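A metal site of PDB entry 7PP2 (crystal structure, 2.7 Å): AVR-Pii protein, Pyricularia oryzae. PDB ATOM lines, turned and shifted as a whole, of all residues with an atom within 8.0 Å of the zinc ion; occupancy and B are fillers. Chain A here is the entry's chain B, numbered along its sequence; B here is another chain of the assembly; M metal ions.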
ATOM      1  N   LYS A  31      -0.082 -24.658  20.585  1.00  0.00           N
ATOM      2  CA  LYS A  31       0.278 -25.131  19.220  1.00  0.00           C
ATOM      3  C   LYS A  31      -0.896 -24.929  18.268  1.00  0.00           C
ATOM      4  O   LYS A  31      -1.981 -25.497  18.534  1.00  0.00           O
ATOM      5  CB  LYS A  31       0.694 -26.605  19.231  1.00  0.00           C
ATOM      6  CG  LYS A  31       2.137 -26.855  18.824  1.00  0.00           C
ATOM      7  CD  LYS A  31       2.395 -26.647  17.352  1.00  0.00           C
ATOM      8  CE  LYS A  31       3.747 -27.186  16.926  1.00  0.00           C
ATOM      9  NZ  LYS A  31       4.852 -26.541  17.675  1.00  0.00           N
ATOM     10  N   CYS A  32      -0.680 -24.174  17.188  1.00  0.00           N
ATOM     11  CA  CYS A  32      -1.688 -23.880  16.138  1.00  0.00           C
ATOM     12  C   CYS A  32      -1.863 -25.112  15.237  1.00  0.00           C
ATOM     13  O   CYS A  32      -0.841 -25.679  14.806  1.00  0.00           O
ATOM     14  CB  CYS A  32      -1.266 -22.678  15.306  1.00  0.00           C
ATOM     15  SG  CYS A  32      -2.501 -22.172  14.094  1.00  0.00           S
ATOM     16  N   SER A  33      -3.117 -25.509  14.996  1.00  0.00           N
ATOM     17  CA  SER A  33      -3.507 -26.570  14.029  1.00  0.00           C
ATOM     18  C   SER A  33      -3.105 -26.152  12.607  1.00  0.00           C
ATOM     19  O   SER A  33      -2.445 -26.954  11.930  1.00  0.00           O
ATOM     20  CB  SER A  33      -4.985 -26.862  14.097  1.00  0.00           C
ATOM     21  OG  SER A  33      -5.347 -27.331  15.387  1.00  0.00           O
ATOM     22  N   LYS A  34      -3.482 -24.932  12.204  1.00  0.00           N
ATOM     23  CA  LYS A  34      -3.388 -24.394  10.820  1.00  0.00           C
ATOM     24  C   LYS A  34      -1.912 -24.200  10.440  1.00  0.00           C
ATOM     25  O   LYS A  34      -1.409 -24.991   9.614  1.00  0.00           O
ATOM     26  CB  LYS A  34      -4.214 -23.112  10.727  1.00  0.00           C
ATOM     27  CG  LYS A  34      -4.305 -22.457   9.350  1.00  0.00           C
ATOM     28  CD  LYS A  34      -5.234 -21.267   9.337  1.00  0.00           C
ATOM     29  CE  LYS A  34      -5.202 -20.499   8.030  1.00  0.00           C
ATOM     30  NZ  LYS A  34      -6.037 -21.154   6.997  1.00  0.00           N
ATOM     31  N   CYS A  35      -1.265 -23.177  11.009  1.00  0.00           N
ATOM     32  CA  CYS A  35       0.202 -22.899  10.860  1.00  0.00           C
ATOM     33  C   CYS A  35       0.951 -23.737  11.898  1.00  0.00           C
ATOM     34  O   CYS A  35       0.283 -24.401  12.712  1.00  0.00           O
ATOM     35  CB  CYS A  35       0.505 -21.431  11.087  1.00  0.00           C
ATOM     36  SG  CYS A  35       0.236 -20.900  12.796  1.00  0.00           S
ATOM     37  N   GLY A  36       2.284 -23.661  11.901  1.00  0.00           N
ATOM     38  CA  GLY A  36       3.117 -24.440  12.842  1.00  0.00           C
ATOM     39  C   GLY A  36       3.191 -23.830  14.238  1.00  0.00           C
ATOM     40  O   GLY A  36       3.686 -24.544  15.131  1.00  0.00           O
ATOM     41  N   TYR A  37       2.717 -22.596  14.439  1.00  0.00           N
ATOM     42  CA  TYR A  37       3.160 -21.689  15.540  1.00  0.00           C
ATOM     43  C   TYR A  37       2.866 -22.293  16.915  1.00  0.00           C
ATOM     44  O   TYR A  37       1.701 -22.630  17.194  1.00  0.00           O
ATOM     45  CB  TYR A  37       2.498 -20.312  15.491  1.00  0.00           C
ATOM     46  CG  TYR A  37       2.983 -19.389  16.589  1.00  0.00           C
ATOM     47  CD1 TYR A  37       2.391 -19.401  17.851  1.00  0.00           C
ATOM     48  CD2 TYR A  37       4.050 -18.525  16.392  1.00  0.00           C
ATOM     49  CE1 TYR A  37       2.843 -18.581  18.875  1.00  0.00           C
ATOM     50  CE2 TYR A  37       4.507 -17.693  17.406  1.00  0.00           C
ATOM     51  CZ  TYR A  37       3.902 -17.724  18.642  1.00  0.00           C
ATOM     52  OH  TYR A  37       4.345 -16.904  19.650  1.00  0.00           O
ATOM     53  N   GLY A  38       3.914 -22.346  17.755  1.00  0.00           N
ATOM     54  CA  GLY A  38       3.862 -22.810  19.152  1.00  0.00           C
ATOM     55  C   GLY A  38       4.600 -21.851  20.086  1.00  0.00           C
ATOM     56  O   GLY A  38       5.561 -21.198  19.637  1.00  0.00           O
ATOM     57  N   TYR A  45       0.714 -16.550  21.755  1.00  0.00           N
ATOM     58  CA  TYR A  45      -0.076 -17.529  20.964  1.00  0.00           C
ATOM     59  C   TYR A  45      -1.341 -16.859  20.420  1.00  0.00           C
ATOM     60  O   TYR A  45      -1.617 -16.998  19.216  1.00  0.00           O
ATOM     61  CB  TYR A  45      -0.471 -18.778  21.758  1.00  0.00           C
ATOM     62  CG  TYR A  45      -1.416 -19.644  20.976  1.00  0.00           C
ATOM     63  CD1 TYR A  45      -0.967 -20.381  19.892  1.00  0.00           C
ATOM     64  CD2 TYR A  45      -2.776 -19.648  21.241  1.00  0.00           C
ATOM     65  CE1 TYR A  45      -1.825 -21.144  19.120  1.00  0.00           C
ATOM     66  CE2 TYR A  45      -3.656 -20.408  20.481  1.00  0.00           C
ATOM     67  CZ  TYR A  45      -3.181 -21.149  19.409  1.00  0.00           C
ATOM     68  OH  TYR A  45      -4.033 -21.898  18.660  1.00  0.00           O
ATOM     69  N   HIS A  48      -0.767 -14.372  17.614  1.00  0.00           N
ATOM     70  CA  HIS A  48       0.004 -14.910  16.463  1.00  0.00           C
ATOM     71  C   HIS A  48      -0.890 -14.898  15.210  1.00  0.00           C
ATOM     72  O   HIS A  48      -2.099 -15.181  15.344  1.00  0.00           O
ATOM     73  CB  HIS A  48       0.531 -16.322  16.761  1.00  0.00           C
ATOM     74  CG  HIS A  48      -0.291 -17.415  16.162  1.00  0.00           C
ATOM     75  ND1 HIS A  48      -1.505 -17.813  16.698  1.00  0.00           N
ATOM     76  CD2 HIS A  48      -0.098 -18.184  15.063  1.00  0.00           C
ATOM     77  CE1 HIS A  48      -2.009 -18.785  15.970  1.00  0.00           C
ATOM     78  NE2 HIS A  48      -1.160 -19.032  14.964  1.00  0.00           N
ATOM     79  N   LYS A  49      -0.305 -14.535  14.073  1.00  0.00           N
ATOM     80  CA  LYS A  49      -0.935 -14.630  12.729  1.00  0.00           C
ATOM     81  C   LYS A  49      -0.525 -15.990  12.123  1.00  0.00           C
ATOM     82  O   LYS A  49       0.660 -16.363  12.257  1.00  0.00           O
ATOM     83  CB  LYS A  49      -0.519 -13.413  11.881  1.00  0.00           C
ATOM     84  CG  LYS A  49      -0.557 -13.594  10.370  1.00  0.00           C
ATOM     85  CD  LYS A  49      -1.927 -13.425   9.749  1.00  0.00           C
ATOM     86  CE  LYS A  49      -2.013 -13.963   8.331  1.00  0.00           C
ATOM     87  NZ  LYS A  49      -0.827 -13.602   7.521  1.00  0.00           N
ATOM     88  N   CYS A  50      -1.475 -16.710  11.527  1.00  0.00           N
ATOM     89  CA  CYS A  50      -1.247 -18.026  10.868  1.00  0.00           C
ATOM     90  C   CYS A  50      -0.356 -17.817   9.639  1.00  0.00           C
ATOM     91  O   CYS A  50      -0.816 -17.151   8.689  1.00  0.00           O
ATOM     92  CB  CYS A  50      -2.555 -18.689  10.469  1.00  0.00           C
ATOM     93  SG  CYS A  50      -3.282 -19.680  11.797  1.00  0.00           S
ATOM     94  N   ASN A  51       0.875 -18.355   9.663  1.00  0.00           N
ATOM     95  CA  ASN A  51       1.863 -18.251   8.551  1.00  0.00           C
ATOM     96  C   ASN A  51       1.896 -19.578   7.784  1.00  0.00           C
ATOM     97  O   ASN A  51       1.245 -20.565   8.135  1.00  0.00           O
ATOM     98  CB  ASN A  51       3.252 -17.867   9.074  1.00  0.00           C
ATOM     99  CG  ASN A  51       3.383 -16.396   9.421  1.00  0.00           C
ATOM    100  OD1 ASN A  51       2.797 -15.538   8.763  1.00  0.00           O
ATOM    101  ND2 ASN A  51       4.161 -16.104  10.445  1.00  0.00           N
ATOM    102  OXT ASN A  51       2.603 -19.692   6.782  1.00  0.00           O
ATOM    103  N   GLU B 332     -11.543 -13.545  15.903  1.00  0.00           N
ATOM    104  CA  GLU B 332     -10.138 -13.994  15.779  1.00  0.00           C
ATOM    105  C   GLU B 332      -9.746 -14.724  17.078  1.00  0.00           C
ATOM    106  O   GLU B 332      -9.064 -15.756  16.989  1.00  0.00           O
ATOM    107  CB  GLU B 332      -9.222 -12.805  15.468  1.00  0.00           C
ATOM    108  CG  GLU B 332      -7.794 -13.189  15.108  1.00  0.00           C
ATOM    109  CD  GLU B 332      -7.611 -13.945  13.795  1.00  0.00           C
ATOM    110  OE1 GLU B 332      -8.487 -13.830  12.906  1.00  0.00           O
ATOM    111  OE2 GLU B 332      -6.590 -14.650  13.670  1.00  0.00           O
ATOM    112  N   LYS B 335     -11.464 -18.039  16.996  1.00  0.00           N
ATOM    113  CA  LYS B 335     -10.815 -18.768  15.869  1.00  0.00           C
ATOM    114  C   LYS B 335      -9.505 -19.387  16.364  1.00  0.00           C
ATOM    115  O   LYS B 335      -9.301 -20.594  16.160  1.00  0.00           O
ATOM    116  CB  LYS B 335     -10.597 -17.815  14.699  1.00  0.00           C
ATOM    117  CG  LYS B 335     -10.211 -18.470  13.381  1.00  0.00           C
ATOM    118  CD  LYS B 335      -8.715 -18.525  13.149  1.00  0.00           C
ATOM    119  CE  LYS B 335      -8.133 -17.203  12.699  1.00  0.00           C
ATOM    120  NZ  LYS B 335      -6.654 -17.238  12.710  1.00  0.00           N
ATOM    121  N   VAL B 336      -8.653 -18.576  17.009  1.00  0.00           N
ATOM    122  CA  VAL B 336      -7.303 -18.986  17.506  1.00  0.00           C
ATOM    123  C   VAL B 336      -7.448 -19.984  18.658  1.00  0.00           C
ATOM    124  O   VAL B 336      -6.599 -20.885  18.768  1.00  0.00           O
ATOM    125  CB  VAL B 336      -6.476 -17.740  17.898  1.00  0.00           C
ATOM    126  CG1 VAL B 336      -5.249 -18.080  18.731  1.00  0.00           C
ATOM    127  CG2 VAL B 336      -6.071 -16.948  16.670  1.00  0.00           C
ATOM    128  N   LEU B 339      -8.315 -23.374  17.185  1.00  0.00           N
ATOM    129  CA  LEU B 339      -7.147 -23.901  16.432  1.00  0.00           C
ATOM    130  C   LEU B 339      -6.119 -24.526  17.383  1.00  0.00           C
ATOM    131  O   LEU B 339      -5.289 -25.312  16.903  1.00  0.00           O
ATOM    132  CB  LEU B 339      -6.521 -22.775  15.598  1.00  0.00           C
ATOM    133  CG  LEU B 339      -7.276 -22.382  14.315  1.00  0.00           C
ATOM    134  CD1 LEU B 339      -6.487 -21.341  13.528  1.00  0.00           C
ATOM    135  CD2 LEU B 339      -7.561 -23.592  13.439  1.00  0.00           C
HETATM  136 ZN    ZN M   1      -1.622 -20.273  13.306  1.00  0.00          ZN
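The side-chain sulfur (SG) of Cys 35 sits close to the backbone NH (N) of Tyr 37, 3.4 Å away. The backbone carbonyl oxygen (O) of Tyr 45 sits at hydrogen-bond distance from a ring nitrogen (ND1) of His 48, 2.6 Å away. The backbone NH (N) of Lys 34 sits close to the side-chain sulfur (SG) of Cys 32 (3.5 Å). The backbone NH of Cys 32 lies within hydrogen-bond range of the backbone carbonyl oxygen of Tyr 37 (2.8 Å).
Four residues have an atom within 4 Å of the zinc ion: Cys 32, Cys 35, His 48 and Cys 50.
The zinc ion is bound by the side-chain sulfur of Cys 35 (2.0 Å), a ring nitrogen (NE2) of His 48 (2.1 Å), the side-chain sulfur of Cys 32 (2.2 Å) and the side-chain sulfur of Cys 50 (2.3 Å). The zinc ion has four donor atoms within binding distance.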
